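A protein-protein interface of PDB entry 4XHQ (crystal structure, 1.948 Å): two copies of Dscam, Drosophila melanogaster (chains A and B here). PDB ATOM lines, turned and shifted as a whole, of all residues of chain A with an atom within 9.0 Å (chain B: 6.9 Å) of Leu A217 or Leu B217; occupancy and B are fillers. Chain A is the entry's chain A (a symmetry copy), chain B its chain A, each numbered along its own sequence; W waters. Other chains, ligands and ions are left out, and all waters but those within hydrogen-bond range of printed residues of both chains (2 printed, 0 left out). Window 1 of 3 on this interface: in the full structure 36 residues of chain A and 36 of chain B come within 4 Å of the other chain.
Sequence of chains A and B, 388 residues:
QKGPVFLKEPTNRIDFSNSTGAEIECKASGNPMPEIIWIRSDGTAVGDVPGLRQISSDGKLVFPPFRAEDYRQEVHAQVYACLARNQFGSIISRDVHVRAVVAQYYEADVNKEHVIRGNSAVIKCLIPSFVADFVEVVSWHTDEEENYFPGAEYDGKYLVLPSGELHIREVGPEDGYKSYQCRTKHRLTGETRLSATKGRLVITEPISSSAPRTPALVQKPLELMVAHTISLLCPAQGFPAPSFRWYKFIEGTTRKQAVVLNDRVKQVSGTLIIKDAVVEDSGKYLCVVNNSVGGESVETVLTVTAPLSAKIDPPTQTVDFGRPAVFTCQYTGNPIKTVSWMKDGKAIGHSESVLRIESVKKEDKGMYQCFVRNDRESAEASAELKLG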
ATOM      1  N   VAL A 122      14.206 -26.666 -34.501  1.00  0.00           N
ATOM      2  CA  VAL A 122      14.958 -27.871 -34.755  1.00  0.00           C
ATOM      3  C   VAL A 122      14.563 -28.896 -33.678  1.00  0.00           C
ATOM      4  O   VAL A 122      14.708 -28.635 -32.481  1.00  0.00           O
ATOM      5  CB  VAL A 122      16.467 -27.580 -34.717  1.00  0.00           C
ATOM      6  CG1 VAL A 122      17.261 -28.875 -34.823  1.00  0.00           C
ATOM      7  CG2 VAL A 122      16.807 -26.580 -35.853  1.00  0.00           C
ATOM      8  N   LYS A 124      15.223 -32.457 -32.048  1.00  0.00           N
ATOM      9  CA  LYS A 124      16.385 -33.313 -31.938  1.00  0.00           C
ATOM     10  C   LYS A 124      16.045 -34.674 -31.375  1.00  0.00           C
ATOM     11  O   LYS A 124      15.332 -34.818 -30.367  1.00  0.00           O
ATOM     12  CB  LYS A 124      17.441 -32.662 -31.037  1.00  0.00           C
ATOM     13  CG  LYS A 124      18.088 -31.407 -31.687  1.00  0.00           C
ATOM     14  CD  LYS A 124      18.861 -30.511 -30.680  1.00  0.00           C
ATOM     15  CE  LYS A 124      17.951 -29.531 -29.915  1.00  0.00           C
ATOM     16  NZ  LYS A 124      17.300 -28.467 -30.768  1.00  0.00           N
ATOM     17  N   LEU A 126      17.527 -37.326 -29.133  1.00  0.00           N
ATOM     18  CA  LEU A 126      18.584 -37.415 -28.123  1.00  0.00           C
ATOM     19  C   LEU A 126      19.020 -38.875 -27.892  1.00  0.00           C
ATOM     20  O   LEU A 126      18.251 -39.680 -27.356  1.00  0.00           O
ATOM     21  CB  LEU A 126      18.103 -36.845 -26.814  1.00  0.00           C
ATOM     22  CG  LEU A 126      17.634 -35.378 -26.988  1.00  0.00           C
ATOM     23  CD1 LEU A 126      17.118 -34.844 -25.676  1.00  0.00           C
ATOM     24  CD2 LEU A 126      18.696 -34.420 -27.562  1.00  0.00           C
ATOM     25  N   SER A 129      25.149 -40.494 -25.082  1.00  0.00           N
ATOM     26  CA  SER A 129      26.513 -40.364 -25.676  1.00  0.00           C
ATOM     27  C   SER A 129      27.216 -41.721 -25.768  1.00  0.00           C
ATOM     28  O   SER A 129      27.966 -41.957 -26.707  1.00  0.00           O
ATOM     29  CB  SER A 129      27.360 -39.414 -24.838  1.00  0.00           C
ATOM     30  OG  SER A 129      27.430 -39.948 -23.513  1.00  0.00           O
ATOM     31  N   GLU A 165      18.595 -34.103 -37.377  1.00  0.00           N
ATOM     32  CA  GLU A 165      17.513 -33.303 -36.795  1.00  0.00           C
ATOM     33  C   GLU A 165      16.348 -33.080 -37.759  1.00  0.00           C
ATOM     34  O   GLU A 165      16.511 -33.135 -38.985  1.00  0.00           O
ATOM     35  CB  GLU A 165      18.030 -31.937 -36.326  1.00  0.00           C
ATOM     36  CG  GLU A 165      19.157 -32.023 -35.300  1.00  0.00           C
ATOM     37  CD  GLU A 165      20.560 -32.104 -35.943  1.00  0.00           C
ATOM     38  OE1 GLU A 165      20.673 -32.326 -37.187  1.00  0.00           O
ATOM     39  OE2 GLU A 165      21.540 -31.939 -35.181  1.00  0.00           O
ATOM     40  N   THR A 214      21.193 -17.535 -28.650  1.00  0.00           N
ATOM     41  CA  THR A 214      21.614 -18.895 -29.019  1.00  0.00           C
ATOM     42  C   THR A 214      21.736 -19.726 -27.716  1.00  0.00           C
ATOM     43  O   THR A 214      21.812 -19.168 -26.605  1.00  0.00           O
ATOM     44  CB  THR A 214      22.976 -18.847 -29.823  1.00  0.00           C
ATOM     45  OG1 THR A 214      23.948 -18.162 -29.031  1.00  0.00           O
ATOM     46  CG2 THR A 214      22.821 -18.042 -31.118  1.00  0.00           C
ATOM     47  N   PRO A 215      21.738 -21.066 -27.824  1.00  0.00           N
ATOM     48  CA  PRO A 215      21.735 -21.860 -26.575  1.00  0.00           C
ATOM     49  C   PRO A 215      23.080 -21.727 -25.848  1.00  0.00           C
ATOM     50  O   PRO A 215      24.053 -21.306 -26.480  1.00  0.00           O
ATOM     51  CB  PRO A 215      21.518 -23.299 -27.058  1.00  0.00           C
ATOM     52  CG  PRO A 215      21.045 -23.191 -28.506  1.00  0.00           C
ATOM     53  CD  PRO A 215      21.635 -21.897 -29.037  1.00  0.00           C
ATOM     54  N   ALA A 216      23.149 -22.113 -24.578  1.00  0.00           N
ATOM     55  CA  ALA A 216      24.420 -22.170 -23.840  1.00  0.00           C
ATOM     56  C   ALA A 216      25.378 -23.242 -24.402  1.00  0.00           C
ATOM     57  O   ALA A 216      26.590 -23.036 -24.451  1.00  0.00           O
ATOM     58  CB  ALA A 216      24.158 -22.450 -22.383  1.00  0.00           C
ATOM     59  N   LEU A 217      24.835 -24.385 -24.820  1.00  0.00           N
ATOM     60  CA  LEU A 217      25.658 -25.478 -25.306  1.00  0.00           C
ATOM     61  C   LEU A 217      25.639 -25.521 -26.828  1.00  0.00           C
ATOM     62  O   LEU A 217      24.569 -25.560 -27.440  1.00  0.00           O
ATOM     63  CB  LEU A 217      25.191 -26.832 -24.713  1.00  0.00           C
ATOM     64  CG  LEU A 217      24.934 -26.795 -23.204  1.00  0.00           C
ATOM     65  CD1 LEU A 217      24.320 -28.126 -22.682  1.00  0.00           C
ATOM     66  CD2 LEU A 217      26.195 -26.561 -22.507  1.00  0.00           C
ATOM     67  N   VAL A 218      26.826 -25.514 -27.441  1.00  0.00           N
ATOM     68  CA  VAL A 218      26.955 -25.398 -28.901  1.00  0.00           C
ATOM     69  C   VAL A 218      27.792 -26.552 -29.436  1.00  0.00           C
ATOM     70  O   VAL A 218      28.501 -27.185 -28.676  1.00  0.00           O
ATOM     71  CB  VAL A 218      27.578 -24.032 -29.292  1.00  0.00           C
ATOM     72  CG1 VAL A 218      26.666 -22.920 -28.855  1.00  0.00           C
ATOM     73  CG2 VAL A 218      28.965 -23.829 -28.667  1.00  0.00           C
ATOM     74  N   GLN A 219      27.683 -26.815 -30.743  1.00  0.00           N
ATOM     75  CA  GLN A 219      28.312 -27.953 -31.400  1.00  0.00           C
ATOM     76  C   GLN A 219      29.832 -27.850 -31.179  1.00  0.00           C
ATOM     77  O   GLN A 219      30.417 -26.860 -31.554  1.00  0.00           O
ATOM     78  CB  GLN A 219      27.978 -27.964 -32.898  1.00  0.00           C
ATOM     79  CG  GLN A 219      28.638 -29.109 -33.710  1.00  0.00           C
ATOM     80  CD  GLN A 219      28.371 -30.466 -33.054  1.00  0.00           C
ATOM     81  OE1 GLN A 219      27.199 -30.868 -32.913  1.00  0.00           O
ATOM     82  NE2 GLN A 219      29.439 -31.173 -32.640  1.00  0.00           N
ATOM     83  N   LYS A 220      30.435 -28.850 -30.547  1.00  0.00           N
ATOM     84  CA  LYS A 220      31.898 -28.915 -30.408  1.00  0.00           C
ATOM     85  C   LYS A 220      32.548 -29.253 -31.804  1.00  0.00           C
ATOM     86  O   LYS A 220      31.830 -29.613 -32.741  1.00  0.00           O
ATOM     87  CB  LYS A 220      32.243 -29.986 -29.358  1.00  0.00           C
ATOM     88  CG  LYS A 220      32.095 -31.407 -29.903  1.00  0.00           C
ATOM     89  CD  LYS A 220      32.620 -32.381 -28.849  1.00  0.00           C
ATOM     90  CE  LYS A 220      32.123 -33.787 -29.036  1.00  0.00           C
ATOM     91  NZ  LYS A 220      32.543 -34.536 -27.791  1.00  0.00           N
ATOM     92  N   PRO A 221      33.908 -29.154 -31.956  1.00  0.00           N
ATOM     93  CA  PRO A 221      34.448 -29.356 -33.318  1.00  0.00           C
ATOM     94  C   PRO A 221      34.032 -30.685 -33.937  1.00  0.00           C
ATOM     95  O   PRO A 221      33.990 -31.725 -33.270  1.00  0.00           O
ATOM     96  CB  PRO A 221      35.977 -29.303 -33.125  1.00  0.00           C
ATOM     97  CG  PRO A 221      36.153 -28.464 -31.884  1.00  0.00           C
ATOM     98  CD  PRO A 221      34.953 -28.791 -30.990  1.00  0.00           C
ATOM     99  N   LEU A 222      33.651 -30.604 -35.207  1.00  0.00           N
ATOM    100  CA  LEU A 222      33.137 -31.706 -35.994  1.00  0.00           C
ATOM    101  C   LEU A 222      34.193 -32.374 -36.854  1.00  0.00           C
ATOM    102  O   LEU A 222      35.028 -31.693 -37.408  1.00  0.00           O
ATOM    103  CB  LEU A 222      32.054 -31.189 -36.926  1.00  0.00           C
ATOM    104  CG  LEU A 222      30.735 -30.843 -36.234  1.00  0.00           C
ATOM    105  CD1 LEU A 222      29.939 -30.004 -37.225  1.00  0.00           C
ATOM    106  CD2 LEU A 222      30.039 -32.157 -35.910  1.00  0.00           C
ATOM    107  N   LEU A 233      24.389 -26.375 -38.039  1.00  0.00           N
ATOM    108  CA  LEU A 233      23.218 -25.638 -37.526  1.00  0.00           C
ATOM    109  C   LEU A 233      23.608 -24.346 -36.872  1.00  0.00           C
ATOM    110  O   LEU A 233      24.718 -24.218 -36.373  1.00  0.00           O
ATOM    111  CB  LEU A 233      22.470 -26.475 -36.465  1.00  0.00           C
ATOM    112  CG  LEU A 233      21.542 -27.535 -37.071  1.00  0.00           C
ATOM    113  CD1 LEU A 233      22.364 -28.471 -37.933  1.00  0.00           C
ATOM    114  CD2 LEU A 233      20.876 -28.334 -35.907  1.00  0.00           C
ATOM    115  N   PRO A 235      21.276 -22.647 -34.122  1.00  0.00           N
ATOM    116  CA  PRO A 235      19.991 -22.478 -33.421  1.00  0.00           C
ATOM    117  C   PRO A 235      19.947 -21.093 -32.809  1.00  0.00           C
ATOM    118  O   PRO A 235      20.913 -20.614 -32.197  1.00  0.00           O
ATOM    119  CB  PRO A 235      20.018 -23.547 -32.304  1.00  0.00           C
ATOM    120  CG  PRO A 235      21.195 -24.486 -32.673  1.00  0.00           C
ATOM    121  CD  PRO A 235      22.169 -23.602 -33.434  1.00  0.00           C
ATOM    122  N   VAL A 298      27.940 -17.366 -33.421  1.00  0.00           N
ATOM    123  CA  VAL A 298      28.514 -18.563 -32.824  1.00  0.00           C
ATOM    124  C   VAL A 298      29.506 -19.143 -33.841  1.00  0.00           C
ATOM    125  O   VAL A 298      29.250 -19.104 -35.064  1.00  0.00           O
ATOM    126  CB  VAL A 298      27.425 -19.629 -32.481  1.00  0.00           C
ATOM    127  CG1 VAL A 298      26.598 -19.930 -33.722  1.00  0.00           C
ATOM    128  CG2 VAL A 298      28.054 -20.959 -31.957  1.00  0.00           C
ATOM    129  N   GLU A 299      30.627 -19.662 -33.337  1.00  0.00           N
ATOM    130  CA  GLU A 299      31.624 -20.323 -34.172  1.00  0.00           C
ATOM    131  C   GLU A 299      31.466 -21.838 -34.162  1.00  0.00           C
ATOM    132  O   GLU A 299      31.202 -22.414 -33.117  1.00  0.00           O
ATOM    133  CB  GLU A 299      33.054 -20.022 -33.684  1.00  0.00           C
ATOM    134  CG  GLU A 299      33.437 -18.572 -33.739  1.00  0.00           C
ATOM    135  CD  GLU A 299      34.883 -18.359 -33.267  1.00  0.00           C
ATOM    136  OE1 GLU A 299      35.555 -19.368 -32.933  1.00  0.00           O
ATOM    137  OE2 GLU A 299      35.341 -17.195 -33.235  1.00  0.00           O
ATOM    138  N   THR A 300      31.689 -22.479 -35.298  1.00  0.00           N
ATOM    139  CA  THR A 300      31.781 -23.956 -35.322  1.00  0.00           C
ATOM    140  C   THR A 300      33.028 -24.356 -36.094  1.00  0.00           C
ATOM    141  O   THR A 300      33.267 -23.848 -37.181  1.00  0.00           O
ATOM    142  CB  THR A 300      30.540 -24.602 -36.002  1.00  0.00           C
ATOM    143  OG1 THR A 300      29.342 -24.148 -35.341  1.00  0.00           O
ATOM    144  CG2 THR A 300      30.627 -26.180 -35.933  1.00  0.00           C
ATOM    145  N   LYS B 124      19.740 -31.071 -15.303  1.00  0.00           N
ATOM    146  CA  LYS B 124      19.685 -29.696 -15.754  1.00  0.00           C
ATOM    147  C   LYS B 124      18.272 -29.156 -15.776  1.00  0.00           C
ATOM    148  O   LYS B 124      17.325 -29.789 -16.272  1.00  0.00           O
ATOM    149  CB  LYS B 124      20.276 -29.576 -17.162  1.00  0.00           C
ATOM    150  CG  LYS B 124      21.813 -29.808 -17.187  1.00  0.00           C
ATOM    151  CD  LYS B 124      22.381 -30.075 -18.608  1.00  0.00           C
ATOM    152  CE  LYS B 124      22.246 -31.545 -19.050  1.00  0.00           C
ATOM    153  NZ  LYS B 124      23.065 -32.531 -18.249  1.00  0.00           N
ATOM    154  N   LEU B 126      16.103 -26.826 -17.806  1.00  0.00           N
ATOM    155  CA  LEU B 126      16.117 -26.235 -19.147  1.00  0.00           C
ATOM    156  C   LEU B 126      15.196 -25.002 -19.228  1.00  0.00           C
ATOM    157  O   LEU B 126      13.970 -25.132 -19.148  1.00  0.00           O
ATOM    158  CB  LEU B 126      15.658 -27.246 -20.165  1.00  0.00           C
ATOM    159  CG  LEU B 126      16.540 -28.519 -20.119  1.00  0.00           C
ATOM    160  CD1 LEU B 126      16.036 -29.531 -21.116  1.00  0.00           C
ATOM    161  CD2 LEU B 126      18.046 -28.274 -20.338  1.00  0.00           C
ATOM    162  N   THR B 214      31.892 -37.506 -24.291  1.00  0.00           N
ATOM    163  CA  THR B 214      31.314 -36.219 -23.874  1.00  0.00           C
ATOM    164  C   THR B 214      30.175 -35.864 -24.863  1.00  0.00           C
ATOM    165  O   THR B 214      30.090 -36.426 -25.971  1.00  0.00           O
ATOM    166  CB  THR B 214      32.437 -35.104 -23.836  1.00  0.00           C
ATOM    167  OG1 THR B 214      33.060 -35.041 -25.121  1.00  0.00           O
ATOM    168  CG2 THR B 214      33.537 -35.466 -22.833  1.00  0.00           C
ATOM    169  N   PRO B 215      29.271 -34.946 -24.477  1.00  0.00           N
ATOM    170  CA  PRO B 215      28.118 -34.694 -25.369  1.00  0.00           C
ATOM    171  C   PRO B 215      28.573 -33.984 -26.651  1.00  0.00           C
ATOM    172  O   PRO B 215      29.676 -33.433 -26.660  1.00  0.00           O
ATOM    173  CB  PRO B 215      27.206 -33.784 -24.538  1.00  0.00           C
ATOM    174  CG  PRO B 215      27.716 -33.875 -23.101  1.00  0.00           C
ATOM    175  CD  PRO B 215      29.195 -34.200 -23.208  1.00  0.00           C
ATOM    176  N   ALA B 216      27.738 -33.957 -27.685  1.00  0.00           N
ATOM    177  CA  ALA B 216      28.013 -33.176 -28.899  1.00  0.00           C
ATOM    178  C   ALA B 216      28.013 -31.656 -28.633  1.00  0.00           C
ATOM    179  O   ALA B 216      28.815 -30.918 -29.206  1.00  0.00           O
ATOM    180  CB  ALA B 216      26.993 -33.496 -29.962  1.00  0.00           C
ATOM    181  N   LEU B 217      27.111 -31.189 -27.770  1.00  0.00           N
ATOM    182  CA  LEU B 217      26.991 -29.767 -27.500  1.00  0.00           C
ATOM    183  C   LEU B 217      27.664 -29.418 -26.180  1.00  0.00           C
ATOM    184  O   LEU B 217      27.365 -30.020 -25.146  1.00  0.00           O
ATOM    185  CB  LEU B 217      25.503 -29.329 -27.491  1.00  0.00           C
ATOM    186  CG  LEU B 217      24.687 -29.868 -28.669  1.00  0.00           C
ATOM    187  CD1 LEU B 217      23.174 -29.533 -28.534  1.00  0.00           C
ATOM    188  CD2 LEU B 217      25.184 -29.279 -29.908  1.00  0.00           C
ATOM    189  N   VAL B 218      28.575 -28.441 -26.215  1.00  0.00           N
ATOM    190  CA  VAL B 218      29.411 -28.106 -25.052  1.00  0.00           C
ATOM    191  C   VAL B 218      29.276 -26.623 -24.734  1.00  0.00           C
ATOM    192  O   VAL B 218      28.838 -25.863 -25.578  1.00  0.00           O
ATOM    193  CB  VAL B 218      30.893 -28.487 -25.310  1.00  0.00           C
ATOM    194  CG1 VAL B 218      31.004 -29.974 -25.501  1.00  0.00           C
ATOM    195  CG2 VAL B 218      31.467 -27.770 -26.541  1.00  0.00           C
ATOM    196  N   GLN B 219      29.645 -26.238 -23.507  1.00  0.00           N
ATOM    197  CA  GLN B 219      29.471 -24.888 -22.991  1.00  0.00           C
ATOM    198  C   GLN B 219      30.233 -23.922 -23.915  1.00  0.00           C
ATOM    199  O   GLN B 219      31.419 -24.081 -24.087  1.00  0.00           O
ATOM    200  CB  GLN B 219      29.991 -24.789 -21.550  1.00  0.00           C
ATOM    201  CG  GLN B 219      29.901 -23.377 -20.914  1.00  0.00           C
ATOM    202  CD  GLN B 219      28.487 -22.808 -21.051  1.00  0.00           C
ATOM    203  OE1 GLN B 219      27.524 -23.405 -20.533  1.00  0.00           O
ATOM    204  NE2 GLN B 219      28.346 -21.667 -21.751  1.00  0.00           N
ATOM    205  N   LYS B 220      29.539 -22.965 -24.519  1.00  0.00           N
ATOM    206  CA  LYS B 220      30.190 -21.910 -25.311  1.00  0.00           C
ATOM    207  C   LYS B 220      30.943 -20.914 -24.347  1.00  0.00           C
ATOM    208  O   LYS B 220      30.752 -20.980 -23.130  1.00  0.00           O
ATOM    209  CB  LYS B 220      29.114 -21.180 -26.135  1.00  0.00           C
ATOM    210  CG  LYS B 220      28.280 -20.219 -25.287  1.00  0.00           C
ATOM    211  CD  LYS B 220      27.364 -19.428 -26.221  1.00  0.00           C
ATOM    212  CE  LYS B 220      26.192 -18.805 -25.518  1.00  0.00           C
ATOM    213  NZ  LYS B 220      25.292 -18.279 -26.615  1.00  0.00           N
ATOM    214  N   PRO B 235      30.860 -32.838 -18.527  1.00  0.00           N
ATOM    215  CA  PRO B 235      29.982 -34.020 -18.560  1.00  0.00           C
ATOM    216  C   PRO B 235      30.658 -35.109 -19.367  1.00  0.00           C
ATOM    217  O   PRO B 235      31.216 -34.874 -20.450  1.00  0.00           O
ATOM    218  CB  PRO B 235      28.709 -33.534 -19.293  1.00  0.00           C
ATOM    219  CG  PRO B 235      28.827 -31.989 -19.323  1.00  0.00           C
ATOM    220  CD  PRO B 235      30.323 -31.716 -19.324  1.00  0.00           C
HETATM  221  O   HOH W   1      35.571 -33.851 -27.162  1.00  0.00           O
HETATM  222  O   HOH W   2      27.065 -16.717 -28.725  1.00  0.00           O
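O of Pro A215 is in hydrogen-bond range of NZ of Lys B220. NZ of Lys A220 lies within hydrogen-bond range of OG1 of Thr B214, 2.8 Å away. O of Pro B215 sits at hydrogen-bond distance from NZ of Lys A220, 3.3 Å away. N of Lys A220 lies within hydrogen-bond range of O of Ala B216 (2.9 Å). The side-chain amide nitrogen (NE2) of Gln A219 lies within hydrogen-bond range of the backbone carbonyl oxygen (O) of Ala B216, at 3.5 Å. The side-chain amide nitrogen of Gln B219 sits at hydrogen-bond distance from the backbone carbonyl oxygen of Ala A216 (3.5 Å). The backbone carbonyl oxygen of Ala A216 sits at hydrogen-bond distance from the backbone NH of Lys B220, at 3.0 Å. The side-chain hydroxyl (OG1) of Thr A214 sits at hydrogen-bond distance from the side-chain amino group (NZ) of Lys B220 (2.8 Å). N of Val B218 is in hydrogen-bond range of O of Val A218.
Among the printed residues, pairs that only touch across the chains: Ala A216 with Val B218 (3.8 Å), Leu A217 with Leu B217 (3.7 Å), Leu A217 with Val B218 (3.2 Å), Leu A217 with Gln B219 (3.6 Å), Val A218 with Ala B216 (3.8 Å), Val A218 with Leu B217 (3.2 Å), Val A218 with Lys B220 (3.7 Å), Gln A219 with Leu B217 (3.6 Å) and Lys A220 with Val B218 (3.7 Å).
Of chain A, only Leu A217 (3.7 Å), Val A218 (3.2 Å) and Gln A219 (3.6 Å) come within 4 Å of Leu B217. Val B218 touches just these residues of chain A: Ala A216, Leu A217, Val A218 and Lys A220. Printed residues of chain A within 4 Å of Thr B214: Lys A220. Of the printed residues of chain B, Ala A216 touches Val B218, Gln B219 and Lys B220. Of the printed residues of chain B, Lys A220 touches Thr B214 (2.8 Å), Pro B215 (3.3 Å), Ala B216 (2.9 Å) and Val B218 (3.7 Å). Of the printed residues of chain B, Gln A219 touches Ala B216 and Leu B217. Lys A124 touches none of the printed residues of chain B. Pro B235 touches none of the printed residues of chain A. The nearest residue of chain A that does not touch Leu B217 is Lys A220 (4.7 Å).
Of the 19 printed residues of chain A, 7 touch a printed residue of chain B. Hydrophobic or aromatic side chains of chain A within 4 Å of the printed part of chain B: Ala A216, Leu A217 and Val A218. Along chain A the printed residues that touch a printed residue of chain B span positions 214 to 220. Hydrophobic or aromatic side chains of chain B that line the printed part of chain A: Ala B216, Leu B217 and Val B218. Along chain B the printed residues that touch a printed residue of chain A span positions 214 to 220. Among the printed residues, 18 pairs touch across the chains. Among the printed residues, no Asp or Glu carboxylate lies within 4 Å of a Lys or Arg side-chain nitrogen of the other chain.
Thr A214 touches Lys B220, and with the chains exchanged Lys A220 touches Thr B214. Ala A216 touches Val B218, and with the chains exchanged Val A218 touches Ala B216. Leu A217 touches Val B218, and with the chains exchanged Val A218 touches Leu B217. Val A218 touches its own counterpart, Val B218. Of the 18 pairs that touch across the chains among the printed residues, 18 have their exchanged pair printed and touching as well.
Water W1 bridges the side-chain amino group of Lys A220 and the side-chain hydroxyl of Thr B214. Water W2 bridges the side-chain amino group of Lys B220 (3.2 Å) and the side-chain hydroxyl of Thr A214 (3.4 Å).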
